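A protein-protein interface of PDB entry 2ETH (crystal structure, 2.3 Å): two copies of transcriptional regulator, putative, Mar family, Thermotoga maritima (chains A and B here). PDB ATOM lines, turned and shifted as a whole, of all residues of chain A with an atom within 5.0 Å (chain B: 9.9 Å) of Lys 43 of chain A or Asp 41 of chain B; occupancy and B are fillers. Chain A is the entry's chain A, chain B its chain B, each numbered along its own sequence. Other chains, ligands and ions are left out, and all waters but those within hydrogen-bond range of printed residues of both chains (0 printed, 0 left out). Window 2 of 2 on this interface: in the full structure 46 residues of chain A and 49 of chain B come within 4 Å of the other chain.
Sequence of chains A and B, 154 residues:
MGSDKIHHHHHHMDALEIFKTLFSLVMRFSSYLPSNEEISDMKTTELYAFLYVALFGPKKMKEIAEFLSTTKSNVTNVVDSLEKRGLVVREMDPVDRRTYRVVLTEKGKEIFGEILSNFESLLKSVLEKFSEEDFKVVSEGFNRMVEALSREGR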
ATOM      1  N   ASP A  41      30.677   3.253  23.825  1.00  0.00           N
ATOM      2  CA  ASP A  41      29.268   2.936  23.850  1.00  0.00           C
ATOM      3  C   ASP A  41      28.722   2.185  22.608  1.00  0.00           C
ATOM      4  O   ASP A  41      27.612   1.682  22.644  1.00  0.00           O
ATOM      5  CB  ASP A  41      28.513   4.244  24.005  1.00  0.00           C
ATOM      6  CG  ASP A  41      27.044   4.037  24.221  1.00  0.00           C
ATOM      7  OD1 ASP A  41      26.686   3.187  25.053  1.00  0.00           O
ATOM      8  OD2 ASP A  41      26.246   4.721  23.552  1.00  0.00           O
ATOM      9  N   MET A  42      29.508   2.102  21.527  1.00  0.00           N
ATOM     10  CA  MET A  42      29.112   1.372  20.314  1.00  0.00           C
ATOM     11  C   MET A  42      29.285  -0.119  20.479  1.00  0.00           C
ATOM     12  O   MET A  42      30.205  -0.552  21.171  1.00  0.00           O
ATOM     13  CB  MET A  42      29.973   1.782  19.115  1.00  0.00           C
ATOM     14  CG  MET A  42      29.726   3.166  18.605  1.00  0.00           C
ATOM     15  SD  MET A  42      30.731   3.481  17.023  1.00  0.00           S
ATOM     16  CE  MET A  42      31.896   4.924  17.596  1.00  0.00           C
ATOM     17  N   LYS A  43      28.435  -0.890  19.795  1.00  0.00           N
ATOM     18  CA  LYS A  43      28.622  -2.331  19.685  1.00  0.00           C
ATOM     19  C   LYS A  43      29.758  -2.633  18.740  1.00  0.00           C
ATOM     20  O   LYS A  43      30.141  -1.815  17.875  1.00  0.00           O
ATOM     21  CB  LYS A  43      27.361  -3.053  19.208  1.00  0.00           C
ATOM     22  CG  LYS A  43      26.114  -2.852  20.112  1.00  0.00           C
ATOM     23  CD  LYS A  43      24.854  -3.381  19.421  1.00  0.00           C
ATOM     24  CE  LYS A  43      23.565  -2.732  19.920  1.00  0.00           C
ATOM     25  NZ  LYS A  43      22.839  -3.523  20.967  1.00  0.00           N
ATOM     26  N   THR A  44      30.295  -3.833  18.902  1.00  0.00           N
ATOM     27  CA  THR A  44      31.464  -4.265  18.162  1.00  0.00           C
ATOM     28  C   THR A  44      31.243  -4.166  16.637  1.00  0.00           C
ATOM     29  O   THR A  44      32.062  -3.583  15.937  1.00  0.00           O
ATOM     30  CB  THR A  44      31.892  -5.710  18.603  1.00  0.00           C
ATOM     31  OG1 THR A  44      30.832  -6.637  18.335  1.00  0.00           O
ATOM     32  CG2 THR A  44      32.207  -5.758  20.114  1.00  0.00           C
ATOM     33  N   THR A  45      30.125  -4.673  16.118  1.00  0.00           N
ATOM     34  CA  THR A  45      29.940  -4.696  14.661  1.00  0.00           C
ATOM     35  C   THR A  45      29.529  -3.313  14.117  1.00  0.00           C
ATOM     36  O   THR A  45      29.812  -2.989  12.972  1.00  0.00           O
ATOM     37  CB  THR A  45      29.006  -5.827  14.182  1.00  0.00           C
ATOM     38  OG1 THR A  45      27.712  -5.620  14.707  1.00  0.00           O
ATOM     39  CG2 THR A  45      29.497  -7.231  14.669  1.00  0.00           C
ATOM     40  N   GLU A  46      28.919  -2.484  14.958  1.00  0.00           N
ATOM     41  CA  GLU A  46      28.691  -1.069  14.618  1.00  0.00           C
ATOM     42  C   GLU A  46      29.993  -0.363  14.351  1.00  0.00           C
ATOM     43  O   GLU A  46      30.109   0.412  13.393  1.00  0.00           O
ATOM     44  CB  GLU A  46      28.013  -0.317  15.788  1.00  0.00           C
ATOM     45  CG  GLU A  46      26.509  -0.283  15.821  1.00  0.00           C
ATOM     46  CD  GLU A  46      25.990   0.187  17.182  1.00  0.00           C
ATOM     47  OE1 GLU A  46      26.646   1.077  17.790  1.00  0.00           O
ATOM     48  OE2 GLU A  46      24.935  -0.343  17.656  1.00  0.00           O
ATOM     49  N   LEU A  47      30.937  -0.534  15.278  1.00  0.00           N
ATOM     50  CA  LEU A  47      32.264   0.099  15.144  1.00  0.00           C
ATOM     51  C   LEU A  47      33.009  -0.405  13.909  1.00  0.00           C
ATOM     52  O   LEU A  47      33.660   0.330  13.223  1.00  0.00           O
ATOM     53  CB  LEU A  47      33.128  -0.145  16.398  1.00  0.00           C
ATOM     54  CG  LEU A  47      34.550   0.450  16.336  1.00  0.00           C
ATOM     55  CD1 LEU A  47      34.501   2.017  16.083  1.00  0.00           C
ATOM     56  CD2 LEU A  47      35.306   0.087  17.623  1.00  0.00           C
ATOM     57  N   ARG A  85      22.801   7.282  16.050  1.00  0.00           N
ATOM     58  CA  ARG A  85      23.856   7.975  16.812  1.00  0.00           C
ATOM     59  C   ARG A  85      24.388   9.195  16.036  1.00  0.00           C
ATOM     60  O   ARG A  85      25.222   9.940  16.544  1.00  0.00           O
ATOM     61  CB  ARG A  85      25.049   7.080  17.158  1.00  0.00           C
ATOM     62  CG  ARG A  85      24.744   5.680  17.547  1.00  0.00           C
ATOM     63  CD  ARG A  85      26.024   4.837  17.690  1.00  0.00           C
ATOM     64  NE  ARG A  85      26.250   4.548  19.103  1.00  0.00           N
ATOM     65  CZ  ARG A  85      25.742   3.511  19.768  1.00  0.00           C
ATOM     66  NH1 ARG A  85      24.984   2.610  19.170  1.00  0.00           N
ATOM     67  NH2 ARG A  85      26.002   3.369  21.051  1.00  0.00           N
ATOM     68  N   SER B  35      31.256 -16.818  13.419  1.00  0.00           N
ATOM     69  CA  SER B  35      30.319 -15.890  14.055  1.00  0.00           C
ATOM     70  C   SER B  35      30.091 -16.266  15.507  1.00  0.00           C
ATOM     71  O   SER B  35      30.026 -17.450  15.844  1.00  0.00           O
ATOM     72  CB  SER B  35      28.965 -15.906  13.320  1.00  0.00           C
ATOM     73  OG  SER B  35      27.882 -15.527  14.166  1.00  0.00           O
ATOM     74  N   ASN B  36      29.977 -15.249  16.356  1.00  0.00           N
ATOM     75  CA  ASN B  36      29.306 -15.395  17.683  1.00  0.00           C
ATOM     76  C   ASN B  36      28.213 -14.303  17.866  1.00  0.00           C
ATOM     77  O   ASN B  36      28.510 -13.109  17.724  1.00  0.00           O
ATOM     78  CB  ASN B  36      30.337 -15.362  18.829  1.00  0.00           C
ATOM     79  N   GLU B  37      26.973 -14.699  18.175  1.00  0.00           N
ATOM     80  CA  GLU B  37      25.823 -13.767  18.142  1.00  0.00           C
ATOM     81  C   GLU B  37      25.645 -12.898  19.367  1.00  0.00           C
ATOM     82  O   GLU B  37      24.775 -12.025  19.378  1.00  0.00           O
ATOM     83  CB  GLU B  37      24.512 -14.531  17.948  1.00  0.00           C
ATOM     84  N   GLU B  38      26.398 -13.176  20.426  1.00  0.00           N
ATOM     85  CA  GLU B  38      26.324 -12.364  21.644  1.00  0.00           C
ATOM     86  C   GLU B  38      27.589 -11.512  21.726  1.00  0.00           C
ATOM     87  O   GLU B  38      27.533 -10.364  22.180  1.00  0.00           O
ATOM     88  CB  GLU B  38      26.129 -13.231  22.892  1.00  0.00           C
ATOM     89  N   ILE B  39      28.719 -12.046  21.259  1.00  0.00           N
ATOM     90  CA  ILE B  39      29.905 -11.220  21.053  1.00  0.00           C
ATOM     91  C   ILE B  39      29.557  -9.995  20.190  1.00  0.00           C
ATOM     92  O   ILE B  39      30.019  -8.875  20.465  1.00  0.00           O
ATOM     93  CB  ILE B  39      31.066 -12.013  20.417  1.00  0.00           C
ATOM     94  N   SER B  40      28.717 -10.193  19.173  1.00  0.00           N
ATOM     95  CA  SER B  40      28.433  -9.122  18.214  1.00  0.00           C
ATOM     96  C   SER B  40      27.437  -8.113  18.782  1.00  0.00           C
ATOM     97  O   SER B  40      27.451  -6.951  18.388  1.00  0.00           O
ATOM     98  CB  SER B  40      27.981  -9.681  16.855  1.00  0.00           C
ATOM     99  OG  SER B  40      26.616  -9.432  16.602  1.00  0.00           O
ATOM    100  N   ASP B  41      26.613  -8.543  19.734  1.00  0.00           N
ATOM    101  CA  ASP B  41      25.644  -7.651  20.365  1.00  0.00           C
ATOM    102  C   ASP B  41      26.274  -6.791  21.460  1.00  0.00           C
ATOM    103  O   ASP B  41      25.722  -5.755  21.827  1.00  0.00           O
ATOM    104  CB  ASP B  41      24.486  -8.476  20.935  1.00  0.00           C
ATOM    105  CG  ASP B  41      23.321  -7.610  21.456  1.00  0.00           C
ATOM    106  OD1 ASP B  41      22.855  -6.703  20.713  1.00  0.00           O
ATOM    107  OD2 ASP B  41      22.852  -7.858  22.601  1.00  0.00           O
ATOM    108  N   MET B  42      27.412  -7.230  21.989  1.00  0.00           N
ATOM    109  CA  MET B  42      28.109  -6.532  23.078  1.00  0.00           C
ATOM    110  C   MET B  42      28.765  -5.209  22.667  1.00  0.00           C
ATOM    111  O   MET B  42      29.371  -5.107  21.619  1.00  0.00           O
ATOM    112  CB  MET B  42      29.187  -7.439  23.690  1.00  0.00           C
ATOM    113  CG  MET B  42      28.698  -8.162  24.916  1.00  0.00           C
ATOM    114  SD  MET B  42      29.935  -9.490  25.615  1.00  0.00           S
ATOM    115  CE  MET B  42      29.737 -10.833  24.330  1.00  0.00           C
ATOM    116  N   LYS B  43      28.653  -4.207  23.526  1.00  0.00           N
ATOM    117  CA  LYS B  43      29.437  -2.989  23.371  1.00  0.00           C
ATOM    118  C   LYS B  43      30.904  -3.296  23.672  1.00  0.00           C
ATOM    119  O   LYS B  43      31.224  -4.306  24.310  1.00  0.00           O
ATOM    120  CB  LYS B  43      28.913  -1.889  24.301  1.00  0.00           C
ATOM    121  CG  LYS B  43      27.566  -1.408  23.927  1.00  0.00           C
ATOM    122  CD  LYS B  43      26.998  -0.552  25.019  1.00  0.00           C
ATOM    123  CE  LYS B  43      25.673   0.081  24.598  1.00  0.00           C
ATOM    124  NZ  LYS B  43      25.256   1.054  25.630  1.00  0.00           N
ATOM    125  N   THR B  44      31.789  -2.421  23.213  1.00  0.00           N
ATOM    126  CA  THR B  44      33.213  -2.751  23.155  1.00  0.00           C
ATOM    127  C   THR B  44      33.845  -2.910  24.533  1.00  0.00           C
ATOM    128  O   THR B  44      34.650  -3.828  24.735  1.00  0.00           O
ATOM    129  CB  THR B  44      34.009  -1.719  22.352  1.00  0.00           C
ATOM    130  OG1 THR B  44      33.707  -0.412  22.831  1.00  0.00           O
ATOM    131  CG2 THR B  44      33.680  -1.803  20.846  1.00  0.00           C
ATOM    132  N   THR B  45      33.474  -2.035  25.475  1.00  0.00           N
ATOM    133  CA  THR B  45      33.945  -2.157  26.855  1.00  0.00           C
ATOM    134  C   THR B  45      33.330  -3.351  27.634  1.00  0.00           C
ATOM    135  O   THR B  45      33.966  -3.862  28.567  1.00  0.00           O
ATOM    136  CB  THR B  45      33.786  -0.834  27.604  1.00  0.00           C
ATOM    137  OG1 THR B  45      32.410  -0.463  27.595  1.00  0.00           O
ATOM    138  CG2 THR B  45      34.567   0.268  26.876  1.00  0.00           C
ATOM    139  N   GLU B  46      32.134  -3.812  27.260  1.00  0.00           N
ATOM    140  CA  GLU B  46      31.549  -5.036  27.850  1.00  0.00           C
ATOM    141  C   GLU B  46      32.286  -6.277  27.433  1.00  0.00           C
ATOM    142  O   GLU B  46      32.589  -7.141  28.259  1.00  0.00           O
ATOM    143  CB  GLU B  46      30.103  -5.215  27.422  1.00  0.00           C
ATOM    144  CG  GLU B  46      29.217  -4.130  27.912  1.00  0.00           C
ATOM    145  CD  GLU B  46      27.810  -4.199  27.349  1.00  0.00           C
ATOM    146  OE1 GLU B  46      27.487  -5.165  26.596  1.00  0.00           O
ATOM    147  OE2 GLU B  46      27.033  -3.260  27.694  1.00  0.00           O
ATOM    148  N   LEU B  47      32.588  -6.354  26.136  1.00  0.00           N
ATOM    149  CA  LEU B  47      33.426  -7.439  25.587  1.00  0.00           C
ATOM    150  C   LEU B  47      34.824  -7.437  26.220  1.00  0.00           C
ATOM    151  O   LEU B  47      35.357  -8.466  26.613  1.00  0.00           O
ATOM    152  CB  LEU B  47      33.529  -7.324  24.066  1.00  0.00           C
ATOM    153  CG  LEU B  47      34.361  -8.414  23.416  1.00  0.00           C
ATOM    154  CD1 LEU B  47      33.792  -9.812  23.793  1.00  0.00           C
ATOM    155  CD2 LEU B  47      34.427  -8.214  21.940  1.00  0.00           C
ATOM    156  N   SER B  81      25.403  -4.858  33.101  1.00  0.00           N
ATOM    157  CA  SER B  81      25.025  -5.235  31.749  1.00  0.00           C
ATOM    158  C   SER B  81      25.471  -6.664  31.365  1.00  0.00           C
ATOM    159  O   SER B  81      24.760  -7.369  30.635  1.00  0.00           O
ATOM    160  CB  SER B  81      25.583  -4.237  30.749  1.00  0.00           C
ATOM    161  OG  SER B  81      25.605  -4.835  29.470  1.00  0.00           O
ATOM    162  N   LEU B  82      26.649  -7.068  31.837  1.00  0.00           N
ATOM    163  CA  LEU B  82      27.136  -8.450  31.639  1.00  0.00           C
ATOM    164  C   LEU B  82      26.352  -9.480  32.476  1.00  0.00           C
ATOM    165  O   LEU B  82      26.242 -10.654  32.114  1.00  0.00           O
ATOM    166  CB  LEU B  82      28.652  -8.546  31.934  1.00  0.00           C
ATOM    167  CG  LEU B  82      29.556  -7.990  30.808  1.00  0.00           C
ATOM    168  CD1 LEU B  82      30.985  -7.902  31.292  1.00  0.00           C
ATOM    169  CD2 LEU B  82      29.452  -8.854  29.561  1.00  0.00           C
ATOM    170  N   LYS B  84      23.006  -8.931  33.330  1.00  0.00           N
ATOM    171  CA  LYS B  84      21.771  -9.002  32.556  1.00  0.00           C
ATOM    172  C   LYS B  84      21.900 -10.042  31.442  1.00  0.00           C
ATOM    173  O   LYS B  84      20.999 -10.861  31.264  1.00  0.00           O
ATOM    174  CB  LYS B  84      21.374  -7.638  31.968  1.00  0.00           C
ATOM    175  CG  LYS B  84      20.306  -6.859  32.772  1.00  0.00           C
ATOM    176  N   ARG B  85      23.031 -10.025  30.727  1.00  0.00           N
ATOM    177  CA  ARG B  85      23.249 -10.916  29.596  1.00  0.00           C
ATOM    178  C   ARG B  85      23.517 -12.372  29.971  1.00  0.00           C
ATOM    179  O   ARG B  85      23.565 -13.232  29.110  1.00  0.00           O
ATOM    180  CB  ARG B  85      24.406 -10.399  28.723  1.00  0.00           C
ATOM    181  CG  ARG B  85      24.145  -9.019  28.168  1.00  0.00           C
ATOM    182  CD  ARG B  85      25.394  -8.352  27.669  1.00  0.00           C
ATOM    183  NE  ARG B  85      25.415  -8.505  26.236  1.00  0.00           N
ATOM    184  CZ  ARG B  85      25.099  -7.563  25.356  1.00  0.00           C
ATOM    185  NH1 ARG B  85      24.807  -6.323  25.724  1.00  0.00           N
ATOM    186  NH2 ARG B  85      25.123  -7.864  24.071  1.00  0.00           N
ATOM    187  N   LEU B  87      26.146 -13.621  31.445  1.00  0.00           N
ATOM    188  CA  LEU B  87      27.506 -13.956  31.100  1.00  0.00           C
ATOM    189  C   LEU B  87      28.412 -13.949  32.321  1.00  0.00           C
ATOM    190  O   LEU B  87      29.416 -14.653  32.350  1.00  0.00           O
ATOM    191  CB  LEU B  87      28.036 -12.975  30.035  1.00  0.00           C
ATOM    192  CG  LEU B  87      27.477 -13.043  28.599  1.00  0.00           C
ATOM    193  CD1 LEU B  87      28.348 -12.227  27.642  1.00  0.00           C
ATOM    194  CD2 LEU B  87      27.361 -14.483  28.102  1.00  0.00           C
ATOM    195  N   LYS B 107      26.754 -20.069  31.095  1.00  0.00           N
ATOM    196  CA  LYS B 107      26.583 -19.470  29.772  1.00  0.00           C
ATOM    197  C   LYS B 107      27.818 -18.657  29.351  1.00  0.00           C
ATOM    198  O   LYS B 107      28.212 -18.656  28.185  1.00  0.00           O
ATOM    199  CB  LYS B 107      25.333 -18.576  29.767  1.00  0.00           C
ATOM    200  CG  LYS B 107      25.118 -17.778  28.486  1.00  0.00           C
ATOM    201  CD  LYS B 107      23.741 -17.158  28.458  1.00  0.00           C
ATOM    202  CE  LYS B 107      23.624 -16.113  27.359  1.00  0.00           C
ATOM    203  NZ  LYS B 107      22.493 -15.172  27.676  1.00  0.00           N
ATOM    204  N   ILE B 111      30.075 -19.532  25.965  1.00  0.00           N
ATOM    205  CA  ILE B 111      30.414 -18.460  25.022  1.00  0.00           C
ATOM    206  C   ILE B 111      31.925 -18.243  24.897  1.00  0.00           C
ATOM    207  O   ILE B 111      32.456 -18.144  23.800  1.00  0.00           O
ATOM    208  CB  ILE B 111      29.721 -17.122  25.419  1.00  0.00           C
ATOM    209  CG1 ILE B 111      28.226 -17.191  25.097  1.00  0.00           C
ATOM    210  CG2 ILE B 111      30.343 -15.927  24.716  1.00  0.00           C
ATOM    211  CD1 ILE B 111      27.948 -17.418  23.617  1.00  0.00           C
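Printed residues of chain B that touch a printed residue of chain A: Ile 39, Ser 40, Asp 41, Met 42, Lys 43, Thr 44 and Leu 47.
The guanidinium group (NH2) of Arg 85 of chain A lies within salt-bridge range of the side-chain carboxylate (OD2) of Asp 41 of chain A (2.9 Å).
The side-chain carboxylate (OE1) of Glu 46 of chain A sits at hydrogen-bond distance from the backbone NH (N) of Lys 43 of chain A, at 3.3 Å.
The side-chain carboxylate (OD2) of Asp 41 of chain B is in salt-bridge range of the guanidinium group (NH2) of Arg 85 of chain B (2.7 Å).
The side-chain carboxylate (OE1) of Glu 46 of chain B lies within hydrogen-bond range of the backbone NH (N) of Lys 43 of chain B (3.4 Å).
The side-chain amino group (NZ) of Lys 43 of chain B lies within salt-bridge range of the side-chain carboxylate (OD1) of Asp 41 of chain A (2.6 Å).
The backbone NH (N) of Thr 44 of chain B lies within hydrogen-bond range of the backbone carbonyl oxygen (O) of Met 42 of chain A, 3.2 Å away.
NZ of Lys 43 of chain A is in salt-bridge range of OD1 of Asp 41 of chain B (3.2 Å).
OG1 of Thr 44 of chain A lies within hydrogen-bond range of O of Ile 39 of chain B, at 3.2 Å.
OG1 of Thr 44 of chain A is in hydrogen-bond range of O of Ser 40 of chain B, at 3.4 Å.
The backbone carbonyl oxygen (O) of Met 42 of chain B lies within hydrogen-bond range of the backbone NH (N) of Thr 44 of chain A (3.1 Å).
Asp 41 of chain A touches Lys 43 of chain B, and with the chains exchanged Lys 43 of chain A touches Asp 41 of chain B.
Met 42 of chain A touches Thr 44 of chain B, and with the chains exchanged Thr 44 of chain A touches Met 42 of chain B.
Lys 43 of chain B touches its own counterpart, Lys 43 of chain A.
Thr 44 of chain A touches Leu 47 of chain B, but with the chains exchanged Leu 47 of chain A does not touch Thr 44 of chain B (4.1 Å).
8 positions are printed for both chains.
Of the 12 pairs that touch across the chains among the printed residues, 7 have their exchanged pair printed and touching as well.
Among the printed residues, pairs that only touch across the chains: Met 42 of chain A with Lys 43 of chain B, Lys 43 of chain A with Ser 40 of chain B, Lys 43 of chain A with Met 42 of chain B, Lys 43 of chain A with Lys 43 of chain B, Thr 44 of chain A with Leu 47 of chain B and Thr 45 of chain A with Ser 40 of chain B.
Printed residues of chain B within 4 Å of Lys 43 of chain A: Ser 40, Asp 41, Met 42 and Lys 43.
Of the printed residues of chain B, Thr 44 of chain A touches Ile 39 (3.2 Å), Ser 40 (3.4 Å), Met 42 (3.1 Å) and Leu 47 (3.8 Å).
No residue of chain B comes within 4 Å of Glu 46 of chain A.
Of the printed residues of chain A, Met 42 of chain B touches Lys 43 (3.5 Å) and Thr 44 (3.1 Å).
Printed residues of chain A within 4 Å of Leu 47 of chain B: Thr 44.
Leu 87 of chain B touches none of the printed residues of chain A.
The nearest printed residue of chain A that does not touch Ser 40 of chain B is Glu 46 of chain A (5.8 Å).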
